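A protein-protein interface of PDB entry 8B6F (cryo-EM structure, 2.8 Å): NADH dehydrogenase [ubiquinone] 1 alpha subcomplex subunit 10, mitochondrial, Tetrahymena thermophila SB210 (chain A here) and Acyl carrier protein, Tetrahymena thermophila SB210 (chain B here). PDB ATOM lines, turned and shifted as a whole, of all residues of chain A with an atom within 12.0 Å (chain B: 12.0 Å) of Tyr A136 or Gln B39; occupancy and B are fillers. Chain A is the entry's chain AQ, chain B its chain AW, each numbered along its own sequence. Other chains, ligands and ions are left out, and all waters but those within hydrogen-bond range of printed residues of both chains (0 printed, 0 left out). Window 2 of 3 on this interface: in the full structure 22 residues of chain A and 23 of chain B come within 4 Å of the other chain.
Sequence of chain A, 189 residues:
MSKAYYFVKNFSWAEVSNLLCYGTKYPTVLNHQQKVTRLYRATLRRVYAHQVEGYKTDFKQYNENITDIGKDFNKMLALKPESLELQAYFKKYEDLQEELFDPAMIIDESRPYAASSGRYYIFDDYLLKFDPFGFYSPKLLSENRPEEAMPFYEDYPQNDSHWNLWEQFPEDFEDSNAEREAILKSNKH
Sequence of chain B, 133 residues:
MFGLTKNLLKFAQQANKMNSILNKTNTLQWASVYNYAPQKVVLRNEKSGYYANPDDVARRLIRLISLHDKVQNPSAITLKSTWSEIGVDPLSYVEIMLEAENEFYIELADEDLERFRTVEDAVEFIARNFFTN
Of the 16 printed residues of chain A, 4 touch a printed residue of chain B. Hydrophobic or aromatic side chains of chain A that line the printed part of chain B: Leu A128 and Tyr A136. Of the 8 printed residues of chain B, 4 touch a printed residue of chain A. Printed residues of chain B that touch a printed residue of chain A: Gln B39, Val B41, Val B42 and Leu B43. Hydrophobic or aromatic side chains of chain B that line the printed part of chain A: Val B41 and Leu B43. Among the printed residues, 7 pairs touch across the chains.
Asp A125 touches Leu B43. Leu A128 touches Val B41 (O to CG1, 3.0 Å). Leu A128 touches Val B42 (CD1 to O, 3.6 Å). Leu A128 touches Leu B43 (CB to CD2, 3.8 Å). CA of Lys A129 touches CG1 of Val B41 (3.99 Å). CG of Lys A129 touches CD2 of Leu B43 (3.5 Å). Gln B39 touches Tyr A136.
Tyr A136 touches just one residue of chain B: Gln B39. Gln B39 touches just one residue of chain A: Tyr A136 (3.1 Å). Asp A131 touches none of the printed residues of chain B. No residue of chain B comes within 4 Å of Gly A134. Ser A137 touches none of the printed residues of chain B. Pro B38 touches none of the printed residues of chain A. Printed residues of chain B within 4 Å of Leu A128: Val B41, Val B42 and Leu B43. Of the printed residues of chain A, Val B41 touches Leu A128 and Lys A129. Tyr A126 touches none of the printed residues of chain B. Leu A140 touches none of the printed residues of chain B.
The side-chain amino group (NZ) of Lys A129 lies within hydrogen-bond range of the backbone carbonyl oxygen (O) of Asp A125, at 2.8 Å. OD2 of Asp A131 lies close to N of Tyr A136.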
ATOM      1  N   ASP A 125       3.038  -8.014  11.759  1.00  0.00           N
ATOM      2  CA  ASP A 125       3.542  -9.202  11.079  1.00  0.00           C
ATOM      3  C   ASP A 125       4.220  -8.854   9.762  1.00  0.00           C
ATOM      4  O   ASP A 125       5.104  -9.588   9.309  1.00  0.00           O
ATOM      5  CB  ASP A 125       2.407 -10.198  10.837  1.00  0.00           C
ATOM      6  CG  ASP A 125       2.116 -11.057  12.050  1.00  0.00           C
ATOM      7  OD1 ASP A 125       3.044 -11.294  12.848  1.00  0.00           O
ATOM      8  OD2 ASP A 125       0.959 -11.502  12.202  1.00  0.00           O
ATOM      9  N   TYR A 126       3.823  -7.750   9.129  1.00  0.00           N
ATOM     10  CA  TYR A 126       4.504  -7.321   7.912  1.00  0.00           C
ATOM     11  C   TYR A 126       5.972  -7.030   8.192  1.00  0.00           C
ATOM     12  O   TYR A 126       6.859  -7.500   7.470  1.00  0.00           O
ATOM     13  CB  TYR A 126       3.813  -6.088   7.330  1.00  0.00           C
ATOM     14  CG  TYR A 126       2.376  -6.320   6.919  1.00  0.00           C
ATOM     15  CD1 TYR A 126       1.992  -7.495   6.286  1.00  0.00           C
ATOM     16  CD2 TYR A 126       1.401  -5.366   7.174  1.00  0.00           C
ATOM     17  CE1 TYR A 126       0.681  -7.710   5.913  1.00  0.00           C
ATOM     18  CE2 TYR A 126       0.087  -5.571   6.805  1.00  0.00           C
ATOM     19  CZ  TYR A 126      -0.267  -6.745   6.175  1.00  0.00           C
ATOM     20  OH  TYR A 126      -1.575  -6.956   5.805  1.00  0.00           O
ATOM     21  N   LEU A 127       6.248  -6.244   9.232  1.00  0.00           N
ATOM     22  CA  LEU A 127       7.635  -5.965   9.594  1.00  0.00           C
ATOM     23  C   LEU A 127       8.349  -7.227  10.057  1.00  0.00           C
ATOM     24  O   LEU A 127       9.528  -7.427   9.747  1.00  0.00           O
ATOM     25  CB  LEU A 127       7.685  -4.891  10.680  1.00  0.00           C
ATOM     26  CG  LEU A 127       7.227  -3.499  10.242  1.00  0.00           C
ATOM     27  CD1 LEU A 127       7.154  -2.564  11.431  1.00  0.00           C
ATOM     28  CD2 LEU A 127       8.153  -2.932   9.180  1.00  0.00           C
ATOM     29  N   LEU A 128       7.656  -8.087  10.807  1.00  0.00           N
ATOM     30  CA  LEU A 128       8.282  -9.312  11.289  1.00  0.00           C
ATOM     31  C   LEU A 128       8.703 -10.209  10.132  1.00  0.00           C
ATOM     32  O   LEU A 128       9.796 -10.785  10.149  1.00  0.00           O
ATOM     33  CB  LEU A 128       7.330 -10.053  12.229  1.00  0.00           C
ATOM     34  CG  LEU A 128       6.895  -9.295  13.489  1.00  0.00           C
ATOM     35  CD1 LEU A 128       5.962 -10.145  14.330  1.00  0.00           C
ATOM     36  CD2 LEU A 128       8.089  -8.847  14.313  1.00  0.00           C
ATOM     37  N   LYS A 129       7.848 -10.338   9.115  1.00  0.00           N
ATOM     38  CA  LYS A 129       8.195 -11.157   7.957  1.00  0.00           C
ATOM     39  C   LYS A 129       9.272 -10.495   7.108  1.00  0.00           C
ATOM     40  O   LYS A 129      10.123 -11.182   6.532  1.00  0.00           O
ATOM     41  CB  LYS A 129       6.954 -11.421   7.105  1.00  0.00           C
ATOM     42  CG  LYS A 129       5.924 -12.325   7.759  1.00  0.00           C
ATOM     43  CD  LYS A 129       4.844 -12.753   6.774  1.00  0.00           C
ATOM     44  CE  LYS A 129       4.158 -11.565   6.116  1.00  0.00           C
ATOM     45  NZ  LYS A 129       3.634 -10.592   7.111  1.00  0.00           N
ATOM     46  N   PHE A 130       9.247  -9.170   7.011  1.00  0.00           N
ATOM     47  CA  PHE A 130      10.143  -8.456   6.110  1.00  0.00           C
ATOM     48  C   PHE A 130      11.591  -8.849   6.357  1.00  0.00           C
ATOM     49  O   PHE A 130      12.106  -8.709   7.469  1.00  0.00           O
ATOM     50  CB  PHE A 130       9.960  -6.949   6.287  1.00  0.00           C
ATOM     51  CG  PHE A 130      10.757  -6.131   5.320  1.00  0.00           C
ATOM     52  CD1 PHE A 130      10.426  -6.111   3.977  1.00  0.00           C
ATOM     53  CD2 PHE A 130      11.827  -5.373   5.753  1.00  0.00           C
ATOM     54  CE1 PHE A 130      11.157  -5.357   3.082  1.00  0.00           C
ATOM     55  CE2 PHE A 130      12.559  -4.616   4.864  1.00  0.00           C
ATOM     56  CZ  PHE A 130      12.224  -4.607   3.527  1.00  0.00           C
ATOM     57  N   ASP A 131      12.243  -9.347   5.310  1.00  0.00           N
ATOM     58  CA  ASP A 131      13.637  -9.762   5.375  1.00  0.00           C
ATOM     59  C   ASP A 131      14.206  -9.835   3.964  1.00  0.00           C
ATOM     60  O   ASP A 131      14.329 -10.931   3.402  1.00  0.00           O
ATOM     61  CB  ASP A 131      13.760 -11.114   6.077  1.00  0.00           C
ATOM     62  CG  ASP A 131      15.199 -11.542   6.266  1.00  0.00           C
ATOM     63  OD1 ASP A 131      16.100 -10.697   6.087  1.00  0.00           O
ATOM     64  OD2 ASP A 131      15.431 -12.724   6.588  1.00  0.00           O
ATOM     65  N   PRO A 132      14.560  -8.701   3.356  1.00  0.00           N
ATOM     66  CA  PRO A 132      15.018  -8.742   1.958  1.00  0.00           C
ATOM     67  C   PRO A 132      16.260  -9.584   1.755  1.00  0.00           C
ATOM     68  O   PRO A 132      16.429 -10.176   0.683  1.00  0.00           O
ATOM     69  CB  PRO A 132      15.270  -7.265   1.629  1.00  0.00           C
ATOM     70  CG  PRO A 132      15.488  -6.611   2.935  1.00  0.00           C
ATOM     71  CD  PRO A 132      14.666  -7.353   3.938  1.00  0.00           C
ATOM     72  N   PHE A 133      17.140  -9.650   2.745  1.00  0.00           N
ATOM     73  CA  PHE A 133      18.328 -10.481   2.663  1.00  0.00           C
ATOM     74  C   PHE A 133      18.044 -11.834   3.309  1.00  0.00           C
ATOM     75  O   PHE A 133      17.084 -11.999   4.064  1.00  0.00           O
ATOM     76  CB  PHE A 133      19.512  -9.785   3.333  1.00  0.00           C
ATOM     77  CG  PHE A 133      19.609  -8.318   3.011  1.00  0.00           C
ATOM     78  CD1 PHE A 133      19.261  -7.843   1.756  1.00  0.00           C
ATOM     79  CD2 PHE A 133      20.030  -7.412   3.967  1.00  0.00           C
ATOM     80  CE1 PHE A 133      19.341  -6.494   1.464  1.00  0.00           C
ATOM     81  CE2 PHE A 133      20.111  -6.065   3.681  1.00  0.00           C
ATOM     82  CZ  PHE A 133      19.767  -5.604   2.428  1.00  0.00           C
ATOM     83  N   GLY A 134      18.889 -12.809   3.002  1.00  0.00           N
ATOM     84  CA  GLY A 134      18.579 -14.183   3.339  1.00  0.00           C
ATOM     85  C   GLY A 134      19.151 -14.689   4.646  1.00  0.00           C
ATOM     86  O   GLY A 134      19.228 -15.904   4.852  1.00  0.00           O
ATOM     87  N   PHE A 135      19.554 -13.790   5.544  1.00  0.00           N
ATOM     88  CA  PHE A 135      20.187 -14.237   6.780  1.00  0.00           C
ATOM     89  C   PHE A 135      19.182 -14.911   7.707  1.00  0.00           C
ATOM     90  O   PHE A 135      19.454 -15.986   8.253  1.00  0.00           O
ATOM     91  CB  PHE A 135      20.864 -13.064   7.485  1.00  0.00           C
ATOM     92  CG  PHE A 135      21.702 -13.480   8.657  1.00  0.00           C
ATOM     93  CD1 PHE A 135      23.007 -13.904   8.470  1.00  0.00           C
ATOM     94  CD2 PHE A 135      21.185 -13.464   9.940  1.00  0.00           C
ATOM     95  CE1 PHE A 135      23.783 -14.295   9.541  1.00  0.00           C
ATOM     96  CE2 PHE A 135      21.956 -13.854  11.016  1.00  0.00           C
ATOM     97  CZ  PHE A 135      23.256 -14.271  10.817  1.00  0.00           C
ATOM     98  N   TYR A 136      18.016 -14.297   7.901  1.00  0.00           N
ATOM     99  CA  TYR A 136      17.004 -14.817   8.816  1.00  0.00           C
ATOM    100  C   TYR A 136      15.943 -15.639   8.098  1.00  0.00           C
ATOM    101  O   TYR A 136      15.598 -16.735   8.549  1.00  0.00           O
ATOM    102  CB  TYR A 136      16.346 -13.660   9.578  1.00  0.00           C
ATOM    103  CG  TYR A 136      17.345 -12.786  10.294  1.00  0.00           C
ATOM    104  CD1 TYR A 136      17.932 -13.201  11.482  1.00  0.00           C
ATOM    105  CD2 TYR A 136      17.717 -11.555   9.774  1.00  0.00           C
ATOM    106  CE1 TYR A 136      18.852 -12.412  12.135  1.00  0.00           C
ATOM    107  CE2 TYR A 136      18.637 -10.758  10.420  1.00  0.00           C
ATOM    108  CZ  TYR A 136      19.202 -11.195  11.599  1.00  0.00           C
ATOM    109  OH  TYR A 136      20.120 -10.405  12.243  1.00  0.00           O
ATOM    110  N   SER A 137      15.416 -15.130   6.986  1.00  0.00           N
ATOM    111  CA  SER A 137      14.468 -15.863   6.162  1.00  0.00           C
ATOM    112  C   SER A 137      15.144 -16.234   4.852  1.00  0.00           C
ATOM    113  O   SER A 137      15.618 -15.334   4.143  1.00  0.00           O
ATOM    114  CB  SER A 137      13.220 -15.022   5.903  1.00  0.00           C
ATOM    115  OG  SER A 137      12.249 -15.758   5.181  1.00  0.00           O
ATOM    116  N   PRO A 138      15.212 -17.513   4.480  1.00  0.00           N
ATOM    117  CA  PRO A 138      16.021 -17.894   3.314  1.00  0.00           C
ATOM    118  C   PRO A 138      15.590 -17.154   2.056  1.00  0.00           C
ATOM    119  O   PRO A 138      14.400 -16.968   1.796  1.00  0.00           O
ATOM    120  CB  PRO A 138      15.785 -19.405   3.193  1.00  0.00           C
ATOM    121  CG  PRO A 138      14.521 -19.660   3.927  1.00  0.00           C
ATOM    122  CD  PRO A 138      14.481 -18.663   5.038  1.00  0.00           C
ATOM    123  N   LYS A 139      16.580 -16.740   1.269  1.00  0.00           N
ATOM    124  CA  LYS A 139      16.370 -15.936   0.073  1.00  0.00           C
ATOM    125  C   LYS A 139      16.734 -16.763  -1.152  1.00  0.00           C
ATOM    126  O   LYS A 139      17.865 -17.248  -1.265  1.00  0.00           O
ATOM    127  CB  LYS A 139      17.212 -14.661   0.131  1.00  0.00           C
ATOM    128  CG  LYS A 139      17.035 -13.719  -1.050  1.00  0.00           C
ATOM    129  CD  LYS A 139      15.655 -13.092  -1.054  1.00  0.00           C
ATOM    130  CE  LYS A 139      15.516 -12.066  -2.167  1.00  0.00           C
ATOM    131  NZ  LYS A 139      16.475 -10.935  -2.018  1.00  0.00           N
ATOM    132  N   LEU A 140      15.782 -16.913  -2.068  1.00  0.00           N
ATOM    133  CA  LEU A 140      16.029 -17.653  -3.297  1.00  0.00           C
ATOM    134  C   LEU A 140      17.035 -16.921  -4.174  1.00  0.00           C
ATOM    135  O   LEU A 140      17.055 -15.690  -4.226  1.00  0.00           O
ATOM    136  CB  LEU A 140      14.722 -17.844  -4.065  1.00  0.00           C
ATOM    137  CG  LEU A 140      13.703 -18.805  -3.461  1.00  0.00           C
ATOM    138  CD1 LEU A 140      12.352 -18.606  -4.113  1.00  0.00           C
ATOM    139  CD2 LEU A 140      14.165 -20.238  -3.628  1.00  0.00           C
ATOM    140  N   TYR B  36      15.970 -17.316  24.793  1.00  0.00           N
ATOM    141  CA  TYR B  36      16.278 -16.298  23.751  1.00  0.00           C
ATOM    142  C   TYR B  36      15.446 -16.542  22.502  1.00  0.00           C
ATOM    143  O   TYR B  36      15.141 -17.683  22.162  1.00  0.00           O
ATOM    144  CB  TYR B  36      17.765 -16.319  23.396  1.00  0.00           C
ATOM    145  CG  TYR B  36      18.681 -16.107  24.577  1.00  0.00           C
ATOM    146  CD1 TYR B  36      19.060 -17.171  25.384  1.00  0.00           C
ATOM    147  CD2 TYR B  36      19.173 -14.846  24.880  1.00  0.00           C
ATOM    148  CE1 TYR B  36      19.898 -16.985  26.462  1.00  0.00           C
ATOM    149  CE2 TYR B  36      20.013 -14.650  25.958  1.00  0.00           C
ATOM    150  CZ  TYR B  36      20.372 -15.722  26.745  1.00  0.00           C
ATOM    151  OH  TYR B  36      21.209 -15.531  27.819  1.00  0.00           O
ATOM    152  N   ALA B  37      15.077 -15.462  21.824  1.00  0.00           N
ATOM    153  CA  ALA B  37      14.311 -15.589  20.597  1.00  0.00           C
ATOM    154  C   ALA B  37      15.166 -16.248  19.516  1.00  0.00           C
ATOM    155  O   ALA B  37      16.350 -15.924  19.378  1.00  0.00           O
ATOM    156  CB  ALA B  37      13.831 -14.219  20.121  1.00  0.00           C
ATOM    157  N   PRO B  38      14.608 -17.175  18.740  1.00  0.00           N
ATOM    158  CA  PRO B  38      15.398 -17.812  17.683  1.00  0.00           C
ATOM    159  C   PRO B  38      15.733 -16.834  16.572  1.00  0.00           C
ATOM    160  O   PRO B  38      15.012 -15.866  16.324  1.00  0.00           O
ATOM    161  CB  PRO B  38      14.482 -18.934  17.181  1.00  0.00           C
ATOM    162  CG  PRO B  38      13.110 -18.444  17.470  1.00  0.00           C
ATOM    163  CD  PRO B  38      13.212 -17.649  18.742  1.00  0.00           C
ATOM    164  N   GLN B  39      16.850 -17.104  15.893  1.00  0.00           N
ATOM    165  CA  GLN B  39      17.257 -16.257  14.780  1.00  0.00           C
ATOM    166  C   GLN B  39      16.270 -16.319  13.621  1.00  0.00           C
ATOM    167  O   GLN B  39      16.293 -15.441  12.753  1.00  0.00           O
ATOM    168  CB  GLN B  39      18.649 -16.662  14.295  1.00  0.00           C
ATOM    169  CG  GLN B  39      19.737 -16.553  15.356  1.00  0.00           C
ATOM    170  CD  GLN B  39      19.991 -15.124  15.798  1.00  0.00           C
ATOM    171  OE1 GLN B  39      19.407 -14.182  15.268  1.00  0.00           O
ATOM    172  NE2 GLN B  39      20.874 -14.958  16.777  1.00  0.00           N
ATOM    173  N   LYS B  40      15.412 -17.333  13.583  1.00  0.00           N
ATOM    174  CA  LYS B  40      14.412 -17.434  12.535  1.00  0.00           C
ATOM    175  C   LYS B  40      13.283 -16.435  12.775  1.00  0.00           C
ATOM    176  O   LYS B  40      13.073 -15.947  13.888  1.00  0.00           O
ATOM    177  CB  LYS B  40      13.850 -18.854  12.465  1.00  0.00           C
ATOM    178  CG  LYS B  40      14.737 -19.842  11.717  1.00  0.00           C
ATOM    179  CD  LYS B  40      16.115 -19.975  12.356  1.00  0.00           C
ATOM    180  CE  LYS B  40      16.937 -21.055  11.669  1.00  0.00           C
ATOM    181  NZ  LYS B  40      18.301 -21.175  12.257  1.00  0.00           N
ATOM    182  N   VAL B  41      12.549 -16.132  11.705  1.00  0.00           N
ATOM    183  CA  VAL B  41      11.466 -15.160  11.787  1.00  0.00           C
ATOM    184  C   VAL B  41      10.295 -15.766  12.548  1.00  0.00           C
ATOM    185  O   VAL B  41       9.812 -16.857  12.215  1.00  0.00           O
ATOM    186  CB  VAL B  41      11.044 -14.707  10.382  1.00  0.00           C
ATOM    187  CG1 VAL B  41       9.808 -13.818  10.447  1.00  0.00           C
ATOM    188  CG2 VAL B  41      12.187 -13.981   9.695  1.00  0.00           C
ATOM    189  N   VAL B  42       9.827 -15.055  13.571  1.00  0.00           N
ATOM    190  CA  VAL B  42       8.696 -15.476  14.388  1.00  0.00           C
ATOM    191  C   VAL B  42       7.626 -14.396  14.314  1.00  0.00           C
ATOM    192  O   VAL B  42       7.931 -13.202  14.403  1.00  0.00           O
ATOM    193  CB  VAL B  42       9.112 -15.734  15.851  1.00  0.00           C
ATOM    194  CG1 VAL B  42       7.928 -16.231  16.666  1.00  0.00           C
ATOM    195  CG2 VAL B  42      10.262 -16.728  15.911  1.00  0.00           C
ATOM    196  N   LEU B  43       6.377 -14.818  14.151  1.00  0.00           N
ATOM    197  CA  LEU B  43       5.249 -13.912  13.997  1.00  0.00           C
ATOM    198  C   LEU B  43       4.430 -13.843  15.281  1.00  0.00           C
ATOM    199  O   LEU B  43       4.540 -14.696  16.165  1.00  0.00           O
ATOM    200  CB  LEU B  43       4.358 -14.356  12.836  1.00  0.00           C
ATOM    201  CG  LEU B  43       5.071 -14.590  11.503  1.00  0.00           C
ATOM    202  CD1 LEU B  43       4.068 -14.979  10.433  1.00  0.00           C
ATOM    203  CD2 LEU B  43       5.859 -13.363  11.080  1.00  0.00           C
